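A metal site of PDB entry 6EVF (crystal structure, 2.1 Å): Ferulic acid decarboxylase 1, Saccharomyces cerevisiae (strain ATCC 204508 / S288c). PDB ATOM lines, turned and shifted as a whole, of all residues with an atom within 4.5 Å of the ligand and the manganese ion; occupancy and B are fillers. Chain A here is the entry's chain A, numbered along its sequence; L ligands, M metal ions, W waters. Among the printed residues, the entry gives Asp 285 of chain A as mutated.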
ATOM      1  N   GLN A 154       9.844  12.307  20.929  1.00  0.00           N
ATOM      2  CA  GLN A 154      10.620  13.428  20.405  1.00  0.00           C
ATOM      3  C   GLN A 154      12.131  13.372  20.806  1.00  0.00           C
ATOM      4  O   GLN A 154      12.525  13.848  21.876  1.00  0.00           O
ATOM      5  CB  GLN A 154       9.900  14.736  20.691  1.00  0.00           C
ATOM      6  CG  GLN A 154      10.673  16.018  20.641  1.00  0.00           C
ATOM      7  CD  GLN A 154      11.446  16.267  19.350  1.00  0.00           C
ATOM      8  OE1 GLN A 154      11.707  15.377  18.615  1.00  0.00           O
ATOM      9  NE2 GLN A 154      11.808  17.534  19.097  1.00  0.00           N
ATOM     10  N   THR A 155      12.951  12.748  19.964  1.00  0.00           N
ATOM     11  CA  THR A 155      14.393  12.866  20.067  1.00  0.00           C
ATOM     12  C   THR A 155      15.071  13.491  18.817  1.00  0.00           C
ATOM     13  O   THR A 155      16.220  13.877  18.897  1.00  0.00           O
ATOM     14  CB  THR A 155      15.014  11.500  20.362  1.00  0.00           C
ATOM     15  OG1 THR A 155      14.661  10.581  19.316  1.00  0.00           O
ATOM     16  CG2 THR A 155      14.532  10.953  21.722  1.00  0.00           C
ATOM     17  N   TYR A 156      14.420  13.524  17.651  1.00  0.00           N
ATOM     18  CA  TYR A 156      15.032  14.125  16.443  1.00  0.00           C
ATOM     19  C   TYR A 156      14.005  14.720  15.499  1.00  0.00           C
ATOM     20  O   TYR A 156      14.106  14.589  14.262  1.00  0.00           O
ATOM     21  CB  TYR A 156      15.821  13.057  15.763  1.00  0.00           C
ATOM     22  CG  TYR A 156      16.963  13.509  14.918  1.00  0.00           C
ATOM     23  CD1 TYR A 156      18.150  13.902  15.483  1.00  0.00           C
ATOM     24  CD2 TYR A 156      16.896  13.460  13.532  1.00  0.00           C
ATOM     25  CE1 TYR A 156      19.209  14.315  14.701  1.00  0.00           C
ATOM     26  CE2 TYR A 156      17.985  13.802  12.733  1.00  0.00           C
ATOM     27  CZ  TYR A 156      19.156  14.215  13.344  1.00  0.00           C
ATOM     28  OH  TYR A 156      20.266  14.596  12.634  1.00  0.00           O
ATOM     29  N   TRP A 168       9.394  36.197  14.686  1.00  0.00           N
ATOM     30  CA  TRP A 168      10.482  35.281  14.920  1.00  0.00           C
ATOM     31  C   TRP A 168       9.857  33.917  15.012  1.00  0.00           C
ATOM     32  O   TRP A 168       8.954  33.726  15.851  1.00  0.00           O
ATOM     33  CB  TRP A 168      11.298  35.697  16.176  1.00  0.00           C
ATOM     34  CG  TRP A 168      12.371  34.720  16.616  1.00  0.00           C
ATOM     35  CD1 TRP A 168      13.033  33.771  15.833  1.00  0.00           C
ATOM     36  CD2 TRP A 168      12.841  34.519  17.945  1.00  0.00           C
ATOM     37  NE1 TRP A 168      13.901  33.043  16.602  1.00  0.00           N
ATOM     38  CE2 TRP A 168      13.800  33.470  17.896  1.00  0.00           C
ATOM     39  CE3 TRP A 168      12.614  35.171  19.170  1.00  0.00           C
ATOM     40  CZ2 TRP A 168      14.525  33.063  19.014  1.00  0.00           C
ATOM     41  CZ3 TRP A 168      13.334  34.781  20.262  1.00  0.00           C
ATOM     42  CH2 TRP A 168      14.271  33.701  20.182  1.00  0.00           C
ATOM     43  N   ASN A 170      11.062  30.063  15.560  1.00  0.00           N
ATOM     44  CA  ASN A 170      12.174  29.281  16.015  1.00  0.00           C
ATOM     45  C   ASN A 170      11.920  27.818  15.727  1.00  0.00           C
ATOM     46  O   ASN A 170      10.840  27.297  16.042  1.00  0.00           O
ATOM     47  CB  ASN A 170      12.396  29.478  17.499  1.00  0.00           C
ATOM     48  CG  ASN A 170      13.774  29.007  17.955  1.00  0.00           C
ATOM     49  OD1 ASN A 170      13.921  27.888  18.458  1.00  0.00           O
ATOM     50  ND2 ASN A 170      14.746  29.838  17.817  1.00  0.00           N
ATOM     51  N   TRP A 171      12.937  27.157  15.146  1.00  0.00           N
ATOM     52  CA  TRP A 171      12.991  25.706  14.978  1.00  0.00           C
ATOM     53  C   TRP A 171      14.045  25.129  15.901  1.00  0.00           C
ATOM     54  O   TRP A 171      15.199  25.530  15.820  1.00  0.00           O
ATOM     55  CB  TRP A 171      13.319  25.361  13.544  1.00  0.00           C
ATOM     56  CG  TRP A 171      12.263  25.760  12.514  1.00  0.00           C
ATOM     57  CD1 TRP A 171      11.023  26.291  12.752  1.00  0.00           C
ATOM     58  CD2 TRP A 171      12.364  25.595  11.073  1.00  0.00           C
ATOM     59  NE1 TRP A 171      10.337  26.451  11.560  1.00  0.00           N
ATOM     60  CE2 TRP A 171      11.143  26.065  10.512  1.00  0.00           C
ATOM     61  CE3 TRP A 171      13.365  25.141  10.231  1.00  0.00           C
ATOM     62  CZ2 TRP A 171      10.889  26.050   9.151  1.00  0.00           C
ATOM     63  CZ3 TRP A 171      13.133  25.124   8.876  1.00  0.00           C
ATOM     64  CH2 TRP A 171      11.897  25.571   8.342  1.00  0.00           C
ATOM     65  N   SER A 172      13.690  24.167  16.738  1.00  0.00           N
ATOM     66  CA  SER A 172      14.657  23.601  17.673  1.00  0.00           C
ATOM     67  C   SER A 172      14.283  22.231  18.126  1.00  0.00           C
ATOM     68  O   SER A 172      13.158  21.799  17.997  1.00  0.00           O
ATOM     69  CB  SER A 172      14.830  24.496  18.914  1.00  0.00           C
ATOM     70  OG  SER A 172      13.637  24.559  19.679  1.00  0.00           O
ATOM     71  N   ILE A 173      15.297  21.538  18.595  1.00  0.00           N
ATOM     72  CA  ILE A 173      15.118  20.208  19.162  1.00  0.00           C
ATOM     73  C   ILE A 173      15.185  20.369  20.704  1.00  0.00           C
ATOM     74  O   ILE A 173      16.108  21.001  21.263  1.00  0.00           O
ATOM     75  CB  ILE A 173      16.237  19.259  18.742  1.00  0.00           C
ATOM     76  CG1 ILE A 173      16.383  19.191  17.226  1.00  0.00           C
ATOM     77  CG2 ILE A 173      16.052  17.879  19.345  1.00  0.00           C
ATOM     78  CD1 ILE A 173      17.258  18.038  16.768  1.00  0.00           C
ATOM     79  N   ALA A 174      14.221  19.728  21.349  1.00  0.00           N
ATOM     80  CA  ALA A 174      14.126  19.502  22.779  1.00  0.00           C
ATOM     81  C   ALA A 174      13.363  18.186  23.009  1.00  0.00           C
ATOM     82  O   ALA A 174      12.402  17.841  22.264  1.00  0.00           O
ATOM     83  CB  ALA A 174      13.362  20.632  23.430  1.00  0.00           C
ATOM     84  N   ARG A 175      13.779  17.439  24.025  1.00  0.00           N
ATOM     85  CA  ARG A 175      13.223  16.124  24.235  1.00  0.00           C
ATOM     86  C   ARG A 175      11.763  16.178  24.658  1.00  0.00           C
ATOM     87  O   ARG A 175      11.356  17.107  25.345  1.00  0.00           O
ATOM     88  CB  ARG A 175      13.999  15.349  25.222  1.00  0.00           C
ATOM     89  CG  ARG A 175      13.832  15.826  26.616  1.00  0.00           C
ATOM     90  CD  ARG A 175      14.841  15.112  27.468  1.00  0.00           C
ATOM     91  NE  ARG A 175      14.469  15.282  28.847  1.00  0.00           N
ATOM     92  CZ  ARG A 175      15.307  15.252  29.871  1.00  0.00           C
ATOM     93  NH1 ARG A 175      16.597  15.097  29.690  1.00  0.00           N
ATOM     94  NH2 ARG A 175      14.817  15.401  31.101  1.00  0.00           N
ATOM     95  N   LEU A 187      11.370  19.116  28.000  1.00  0.00           N
ATOM     96  CA  LEU A 187      12.153  20.282  28.471  1.00  0.00           C
ATOM     97  C   LEU A 187      11.858  21.525  27.653  1.00  0.00           C
ATOM     98  O   LEU A 187      11.975  21.486  26.426  1.00  0.00           O
ATOM     99  CB  LEU A 187      13.634  20.005  28.333  1.00  0.00           C
ATOM    100  CG  LEU A 187      14.301  18.953  29.227  1.00  0.00           C
ATOM    101  CD1 LEU A 187      15.827  18.993  29.076  1.00  0.00           C
ATOM    102  CD2 LEU A 187      13.930  19.157  30.681  1.00  0.00           C
ATOM    103  N   ILE A 189      13.368  24.913  28.779  1.00  0.00           N
ATOM    104  CA  ILE A 189      14.188  25.500  29.856  1.00  0.00           C
ATOM    105  C   ILE A 189      14.992  26.670  29.364  1.00  0.00           C
ATOM    106  O   ILE A 189      15.431  26.706  28.201  1.00  0.00           O
ATOM    107  CB  ILE A 189      15.159  24.478  30.487  1.00  0.00           C
ATOM    108  CG1 ILE A 189      16.148  23.882  29.458  1.00  0.00           C
ATOM    109  CG2 ILE A 189      14.367  23.372  31.149  1.00  0.00           C
ATOM    110  CD1 ILE A 189      17.472  23.379  30.039  1.00  0.00           C
ATOM    111  N   GLN A 192      17.073  28.342  26.484  1.00  0.00           N
ATOM    112  CA  GLN A 192      16.682  27.891  25.167  1.00  0.00           C
ATOM    113  C   GLN A 192      15.588  28.760  24.537  1.00  0.00           C
ATOM    114  O   GLN A 192      14.747  29.346  25.225  1.00  0.00           O
ATOM    115  CB  GLN A 192      16.265  26.415  25.197  1.00  0.00           C
ATOM    116  CG  GLN A 192      17.318  25.470  25.812  1.00  0.00           C
ATOM    117  CD  GLN A 192      18.547  25.353  24.919  1.00  0.00           C
ATOM    118  OE1 GLN A 192      19.354  26.292  24.841  1.00  0.00           O
ATOM    119  NE2 GLN A 192      18.638  24.256  24.150  1.00  0.00           N
ATOM    120  N   HIS A 193      15.650  28.917  23.214  1.00  0.00           N
ATOM    121  CA  HIS A 193      14.711  29.785  22.528  1.00  0.00           C
ATOM    122  C   HIS A 193      13.255  29.347  22.586  1.00  0.00           C
ATOM    123  O   HIS A 193      12.385  30.191  22.530  1.00  0.00           O
ATOM    124  CB  HIS A 193      15.135  30.099  21.127  1.00  0.00           C
ATOM    125  CG  HIS A 193      16.415  30.866  21.064  1.00  0.00           C
ATOM    126  ND1 HIS A 193      17.226  30.868  19.941  1.00  0.00           N
ATOM    127  CD2 HIS A 193      17.006  31.677  21.976  1.00  0.00           C
ATOM    128  CE1 HIS A 193      18.262  31.654  20.180  1.00  0.00           C
ATOM    129  NE2 HIS A 193      18.163  32.150  21.397  1.00  0.00           N
ATOM    130  N   ILE A 194      13.022  28.067  22.712  1.00  0.00           N
ATOM    131  CA  ILE A 194      11.722  27.517  22.887  1.00  0.00           C
ATOM    132  C   ILE A 194      11.077  28.071  24.185  1.00  0.00           C
ATOM    133  O   ILE A 194       9.929  28.459  24.132  1.00  0.00           O
ATOM    134  CB  ILE A 194      11.752  25.966  22.864  1.00  0.00           C
ATOM    135  CG1 ILE A 194      10.326  25.426  22.688  1.00  0.00           C
ATOM    136  CG2 ILE A 194      12.516  25.385  24.046  1.00  0.00           C
ATOM    137  CD1 ILE A 194      10.209  23.915  22.668  1.00  0.00           C
ATOM    138  N   SER A 226      18.127  23.143  13.553  1.00  0.00           N
ATOM    139  CA  SER A 226      17.348  22.986  14.799  1.00  0.00           C
ATOM    140  C   SER A 226      18.197  22.729  16.059  1.00  0.00           C
ATOM    141  O   SER A 226      17.824  23.199  17.175  1.00  0.00           O
ATOM    142  CB  SER A 226      16.241  21.933  14.644  1.00  0.00           C
ATOM    143  OG  SER A 226      15.325  22.318  13.615  1.00  0.00           O
ATOM    144  N   SER A 227      19.326  22.037  15.905  1.00  0.00           N
ATOM    145  CA  SER A 227      20.241  21.766  17.026  1.00  0.00           C
ATOM    146  C   SER A 227      21.328  22.814  17.231  1.00  0.00           C
ATOM    147  O   SER A 227      22.201  22.623  18.092  1.00  0.00           O
ATOM    148  CB  SER A 227      20.931  20.458  16.848  1.00  0.00           C
ATOM    149  OG  SER A 227      21.681  20.147  18.026  1.00  0.00           O
ATOM    150  N   MET A 228      21.300  23.883  16.447  1.00  0.00           N
ATOM    151  CA  MET A 228      22.331  24.873  16.469  1.00  0.00           C
ATOM    152  C   MET A 228      21.964  26.139  17.216  1.00  0.00           C
ATOM    153  O   MET A 228      20.888  26.681  16.987  1.00  0.00           O
ATOM    154  CB  MET A 228      22.676  25.208  15.023  1.00  0.00           C
ATOM    155  CG  MET A 228      23.782  26.188  14.877  1.00  0.00           C
ATOM    156  SD  MET A 228      24.145  26.311  13.098  1.00  0.00           S
ATOM    157  CE  MET A 228      25.571  27.372  13.201  1.00  0.00           C
ATOM    158  N   PRO A 229      22.863  26.668  18.063  1.00  0.00           N
ATOM    159  CA  PRO A 229      22.531  27.886  18.803  1.00  0.00           C
ATOM    160  C   PRO A 229      22.777  29.159  18.014  1.00  0.00           C
ATOM    161  O   PRO A 229      23.684  29.997  18.313  1.00  0.00           O
ATOM    162  CB  PRO A 229      23.398  27.749  20.091  1.00  0.00           C
ATOM    163  CG  PRO A 229      24.597  27.033  19.640  1.00  0.00           C
ATOM    164  CD  PRO A 229      24.123  26.061  18.570  1.00  0.00           C
ATOM    165  N   ILE A 230      21.958  29.347  17.001  1.00  0.00           N
ATOM    166  CA  ILE A 230      22.025  30.591  16.285  1.00  0.00           C
ATOM    167  C   ILE A 230      21.388  31.749  17.107  1.00  0.00           C
ATOM    168  O   ILE A 230      20.752  31.527  18.141  1.00  0.00           O
ATOM    169  CB  ILE A 230      21.428  30.472  14.865  1.00  0.00           C
ATOM    170  CG1 ILE A 230      19.923  30.321  14.888  1.00  0.00           C
ATOM    171  CG2 ILE A 230      22.042  29.362  14.079  1.00  0.00           C
ATOM    172  CD1 ILE A 230      19.310  30.366  13.481  1.00  0.00           C
ATOM    173  N   GLU A 236      15.326  30.209  12.221  1.00  0.00           N
ATOM    174  CA  GLU A 236      16.180  29.168  11.649  1.00  0.00           C
ATOM    175  C   GLU A 236      15.886  28.892  10.158  1.00  0.00           C
ATOM    176  O   GLU A 236      16.818  28.646   9.386  1.00  0.00           O
ATOM    177  CB  GLU A 236      15.968  27.883  12.378  1.00  0.00           C
ATOM    178  CG  GLU A 236      16.748  27.725  13.639  1.00  0.00           C
ATOM    179  CD  GLU A 236      16.223  28.550  14.823  1.00  0.00           C
ATOM    180  OE1 GLU A 236      15.127  29.165  14.789  1.00  0.00           O
ATOM    181  OE2 GLU A 236      16.931  28.502  15.820  1.00  0.00           O
ATOM    182  N   PHE A 283      15.783  10.953  31.487  1.00  0.00           N
ATOM    183  CA  PHE A 283      16.095  10.480  30.145  1.00  0.00           C
ATOM    184  C   PHE A 283      17.581  10.215  30.037  1.00  0.00           C
ATOM    185  O   PHE A 283      18.378  11.002  30.491  1.00  0.00           O
ATOM    186  CB  PHE A 283      15.716  11.540  29.129  1.00  0.00           C
ATOM    187  CG  PHE A 283      15.865  11.092  27.696  1.00  0.00           C
ATOM    188  CD1 PHE A 283      15.252   9.911  27.261  1.00  0.00           C
ATOM    189  CD2 PHE A 283      16.653  11.805  26.808  1.00  0.00           C
ATOM    190  CE1 PHE A 283      15.395   9.483  25.951  1.00  0.00           C
ATOM    191  CE2 PHE A 283      16.767  11.405  25.510  1.00  0.00           C
ATOM    192  CZ  PHE A 283      16.147  10.250  25.078  1.00  0.00           C
ATOM    193  N   ASP A 285      20.919  10.618  28.782  1.00  0.00           N
ATOM    194  CA  ASP A 285      21.324  11.845  28.125  1.00  0.00           C
ATOM    195  C   ASP A 285      22.768  11.880  27.606  1.00  0.00           C
ATOM    196  O   ASP A 285      23.413  10.841  27.482  1.00  0.00           O
ATOM    197  CB  ASP A 285      20.879  13.094  28.894  1.00  0.00           C
ATOM    198  CG  ASP A 285      20.317  14.211  27.898  1.00  0.00           C
ATOM    199  OD1 ASP A 285      20.765  14.253  26.706  1.00  0.00           O
ATOM    200  OD2 ASP A 285      19.432  14.994  28.276  1.00  0.00           O
ATOM    201  N   SER A 317      17.197   9.694  17.932  1.00  0.00           N
ATOM    202  CA  SER A 317      18.511   9.670  18.571  1.00  0.00           C
ATOM    203  C   SER A 317      18.373   9.044  19.975  1.00  0.00           C
ATOM    204  O   SER A 317      17.407   9.299  20.721  1.00  0.00           O
ATOM    205  CB  SER A 317      19.056  11.097  18.681  1.00  0.00           C
ATOM    206  OG  SER A 317      20.291  11.172  19.406  1.00  0.00           O
ATOM    207  N   PRO A 319      20.586   8.911  23.081  1.00  0.00           N
ATOM    208  CA  PRO A 319      21.881   9.440  23.580  1.00  0.00           C
ATOM    209  C   PRO A 319      22.540   8.602  24.628  1.00  0.00           C
ATOM    210  O   PRO A 319      21.880   7.767  25.304  1.00  0.00           O
ATOM    211  CB  PRO A 319      21.517  10.808  24.176  1.00  0.00           C
ATOM    212  CG  PRO A 319      20.157  11.142  23.675  1.00  0.00           C
ATOM    213  CD  PRO A 319      19.465   9.797  23.472  1.00  0.00           C
ATOM    214  N   GLU A 325      24.291  11.838  18.361  1.00  0.00           N
ATOM    215  CA  GLU A 325      23.964  13.157  17.859  1.00  0.00           C
ATOM    216  C   GLU A 325      24.169  14.270  18.919  1.00  0.00           C
ATOM    217  O   GLU A 325      24.370  15.444  18.575  1.00  0.00           O
ATOM    218  CB  GLU A 325      22.513  13.221  17.414  1.00  0.00           C
ATOM    219  CG  GLU A 325      22.217  12.393  16.185  1.00  0.00           C
ATOM    220  CD  GLU A 325      22.060  10.880  16.387  1.00  0.00           C
ATOM    221  OE1 GLU A 325      21.797  10.405  17.549  1.00  0.00           O
ATOM    222  OE2 GLU A 325      22.252  10.203  15.338  1.00  0.00           O
ATOM    223  N   THR A 326      24.075  13.895  20.195  1.00  0.00           N
ATOM    224  CA  THR A 326      24.290  14.863  21.252  1.00  0.00           C
ATOM    225  C   THR A 326      25.787  15.300  21.292  1.00  0.00           C
ATOM    226  O   THR A 326      26.140  16.258  21.979  1.00  0.00           O
ATOM    227  CB  THR A 326      23.790  14.338  22.630  1.00  0.00           C
ATOM    228  OG1 THR A 326      24.578  13.230  23.071  1.00  0.00           O
ATOM    229  CG2 THR A 326      22.316  13.966  22.597  1.00  0.00           C
ATOM    230  N   LEU A 329      26.168  16.634  16.808  1.00  0.00           N
ATOM    231  CA  LEU A 329      25.419  17.862  16.501  1.00  0.00           C
ATOM    232  C   LEU A 329      25.516  18.881  17.596  1.00  0.00           C
ATOM    233  O   LEU A 329      25.869  20.031  17.366  1.00  0.00           O
ATOM    234  CB  LEU A 329      23.940  17.582  16.144  1.00  0.00           C
ATOM    235  CG  LEU A 329      23.719  16.637  15.005  1.00  0.00           C
ATOM    236  CD1 LEU A 329      22.226  16.483  14.728  1.00  0.00           C
ATOM    237  CD2 LEU A 329      24.475  17.095  13.782  1.00  0.00           C
ATOM    238  N   ILE A 330      25.162  18.506  18.816  1.00  0.00           N
ATOM    239  CA  ILE A 330      25.110  19.500  19.899  1.00  0.00           C
ATOM    240  C   ILE A 330      26.506  20.075  20.030  1.00  0.00           C
ATOM    241  O   ILE A 330      26.668  21.275  19.912  1.00  0.00           O
ATOM    242  CB  ILE A 330      24.587  18.987  21.251  1.00  0.00           C
ATOM    243  CG1 ILE A 330      23.185  18.431  21.129  1.00  0.00           C
ATOM    244  CG2 ILE A 330      24.498  20.112  22.264  1.00  0.00           C
ATOM    245  CD1 ILE A 330      22.592  18.021  22.453  1.00  0.00           C
ATOM    246  N   LYS A 394      24.888  32.066  26.096  1.00  0.00           N
ATOM    247  CA  LYS A 394      24.102  30.870  25.736  1.00  0.00           C
ATOM    248  C   LYS A 394      24.950  29.813  25.048  1.00  0.00           C
ATOM    249  O   LYS A 394      24.836  28.662  25.342  1.00  0.00           O
ATOM    250  CB  LYS A 394      22.910  31.239  24.863  1.00  0.00           C
ATOM    251  CG  LYS A 394      22.097  30.068  24.314  1.00  0.00           C
ATOM    252  CD  LYS A 394      20.751  30.647  23.835  1.00  0.00           C
ATOM    253  CE  LYS A 394      19.869  29.573  23.186  1.00  0.00           C
ATOM    254  NZ  LYS A 394      20.520  29.002  21.964  1.00  0.00           N
HETATM  255  C1  LIG L   1      19.810  18.470  20.536  1.00  0.00           C
HETATM  256  C2  LIG L   1      19.862  17.251  19.890  1.00  0.00           C
HETATM  257  C3  LIG L   1      19.296  16.082  20.431  1.00  0.00           C
HETATM  258  C4  LIG L   1      18.278  19.915  23.515  1.00  0.00           C
HETATM  259  C5  LIG L   1      18.726  16.106  21.763  1.00  0.00           C
HETATM  260  N1  LIG L   1      16.535  20.232  25.532  1.00  0.00           N
HETATM  261  C6  LIG L   1      17.093  21.281  24.977  1.00  0.00           C
HETATM  262  C7  LIG L   1      18.508  13.549  22.127  1.00  0.00           C
HETATM  263  C8  LIG L   1      18.073  14.988  22.477  1.00  0.00           C
HETATM  264  C9  LIG L   1      18.120  16.364  24.599  1.00  0.00           C
HETATM  265  O1  LIG L   1      16.677  22.427  25.462  1.00  0.00           O
HETATM  266  N2  LIG L   1      18.001  21.161  23.979  1.00  0.00           N
HETATM  267  C10 LIG L   1      16.786  18.968  25.088  1.00  0.00           C
HETATM  268  O2  LIG L   1      16.154  18.034  25.616  1.00  0.00           O
HETATM  269  C11 LIG L   1      17.690  18.751  24.086  1.00  0.00           C
HETATM  270  N3  LIG L   1      18.162  17.514  23.745  1.00  0.00           N
HETATM  271  C12 LIG L   1      18.116  15.122  23.945  1.00  0.00           C
HETATM  272  C13 LIG L   1      16.600  14.983  22.117  1.00  0.00           C
HETATM  273  C14 LIG L   1      18.701  17.377  22.414  1.00  0.00           C
HETATM  274  C15 LIG L   1      19.399  14.868  19.513  1.00  0.00           C
HETATM  275  C16 LIG L   1      20.507  17.293  18.549  1.00  0.00           C
HETATM  276  C17 LIG L   1      19.267  18.546  21.809  1.00  0.00           C
HETATM  277  N4  LIG L   1      19.232  19.780  22.499  1.00  0.00           N
HETATM  278  C18 LIG L   1      19.870  21.025  22.093  1.00  0.00           C
HETATM  279  C19 LIG L   1      19.125  22.091  21.325  1.00  0.00           C
HETATM  280  O3  LIG L   1      18.522  21.472  20.216  1.00  0.00           O
HETATM  281  C20 LIG L   1      20.176  23.125  20.988  1.00  0.00           C
HETATM  282  O4  LIG L   1      20.614  23.703  22.233  1.00  0.00           O
HETATM  283  C21 LIG L   1      19.650  24.226  20.089  1.00  0.00           C
HETATM  284  O5  LIG L   1      20.645  25.236  19.986  1.00  0.00           O
HETATM  285  C22 LIG L   1      18.372  24.817  20.642  1.00  0.00           C
HETATM  286  O6  LIG L   1      17.762  25.702  19.734  1.00  0.00           O
HETATM  287  P1  LIG L   1      17.663  27.276  20.054  1.00  0.00           P
HETATM  288  O7  LIG L   1      16.763  27.713  18.952  1.00  0.00           O
HETATM  289  O8  LIG L   1      17.011  27.371  21.404  1.00  0.00           O
HETATM  290  O9  LIG L   1      19.053  27.799  19.944  1.00  0.00           O
HETATM  291 MN    MN M   1      16.871  29.665  17.814  1.00  0.00          MN
HETATM  292  O   HOH W   1      23.263  23.627  22.104  1.00  0.00           O
HETATM  293  O   HOH W   2      14.300  23.231  26.396  1.00  0.00           O
HETATM  294  O   HOH W   3      17.162  31.781  16.782  1.00  0.00           O
HETATM  295  O   HOH W   4      21.258  26.512  23.026  1.00  0.00           O
HETATM  296  O   HOH W   5      19.242  29.359  17.951  1.00  0.00           O
HETATM  297  O   HOH W   6      15.789  23.240  22.723  1.00  0.00           O
HETATM  298  O   HOH W   7      14.924  25.846  21.801  1.00  0.00           O
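An oxygen (O4) of the ligand sits at hydrogen-bond distance from the side-chain amide nitrogen of Gln 192 (2.8 Å).
O of Met 228 sits close to O5 of the ligand (3.3 Å).
The backbone NH of His 193 is in hydrogen-bond range of an oxygen (O8) of the ligand (2.7 Å).
The side-chain amino group (NZ) of Lys 394 lies within salt-bridge range of an oxygen (O9) of the ligand.
An oxygen (O2) of the ligand lies within hydrogen-bond range of the backbone NH (N) of Arg 175 (2.9 Å).
The backbone carbonyl oxygen (O) of Ile 173 sits at hydrogen-bond distance from an oxygen (O3) of the ligand, 2.7 Å away.
The backbone carbonyl oxygen (O) of Arg 175 lies within hydrogen-bond range of the backbone NH (N) of Leu 187, at 3.3 Å.
O of Ala 174 lies close to NE2 of Gln 154 (3.2 Å).
N of Ile 173 sits at hydrogen-bond distance from O of Ser 226 (3.3 Å).
The side-chain carboxylate (OD2) of Asp 285 is in salt-bridge range of the guanidinium group (NH1) of Arg 175, 3.2 Å away.
The side-chain hydroxyl (OG) of Ser 317 is in hydrogen-bond range of the side-chain carboxylate (OE1) of Glu 325 (2.5 Å).
OG1 of Thr 155 lies within hydrogen-bond range of N of Ser 317 (3.0 Å).
O of Glu 325 sits at hydrogen-bond distance from N of Ile 330 (3.2 Å).
The backbone NH (N) of Trp 171 is in hydrogen-bond range of the side-chain carboxylate (OE1) of Glu 236 (3.0 Å).
N of Pro 229 lies close to O5 of the ligand (3.3 Å).
O of Thr 155 touches C15 of the ligand (3.4 Å).
Ser 172 touches the ligand.
Ala 174 touches the ligand.
Leu 187 touches the ligand.
O of Ser 226 touches O3 of the ligand, at 3.6 Å.
Ser 227 touches the ligand.
Asp 285 touches the ligand (OD1 to C12, 3.9 Å).
Ser 317 touches the ligand (OG to C15, 3.8 Å).
Pro 319 touches the ligand (CG to C7, 3.3 Å).
Thr 326 touches the ligand (CG2 to C7, 3.9 Å).
Ile 330 touches the ligand.
Hydrophobic or aromatic side chains within 4 Å of the ligand: Ile 173, Ala 174, Leu 187, His 193, Pro 229, Pro 319 and Ile 330.
Of the 30 residues printed, 20 come within 4 Å of the ligand.
Along chain A the residues within 4 Å of the ligand span positions 155 to 394.
Three residues have an atom within 4 Å of the manganese ion: Asn 170, His 193 and Glu 236.
The manganese ion is bound by the side-chain amide nitrogen of Asn 170, an oxygen (O7) of the ligand, the side-chain carboxylate of Glu 236, water W3, water W5 and a ring nitrogen (ND1) of His 193.
Water W5 lies within hydrogen-bond range of an oxygen (O9) of the ligand, the backbone carbonyl oxygen (O) of Ile 230 and the backbone carbonyl oxygen (O) of Met 228.
Water W7 lies within hydrogen-bond range of O8 of the ligand (2.6 Å), OG of Ser 172 (2.8 Å), N of Ile 194 (3.1 Å) and N of His 193 (3.5 Å).
Water W2 lies within hydrogen-bond range of an oxygen (O1) of the ligand (2.7 Å), the backbone carbonyl oxygen of Leu 187 (2.9 Å) and the backbone NH of Ile 189 (3.1 Å).
Water W4 lies within hydrogen-bond range of the side-chain amide oxygen (OE1) of Gln 192, the side-chain amino group (NZ) of Lys 394 and an oxygen (O4) of the ligand.
Water W6 lies within hydrogen-bond range of the backbone carbonyl oxygen (O) of Ile 173 (2.7 Å), an oxygen (O1) of the ligand (3.0 Å) and the side-chain amide nitrogen (NE2) of Gln 192 (3.3 Å).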
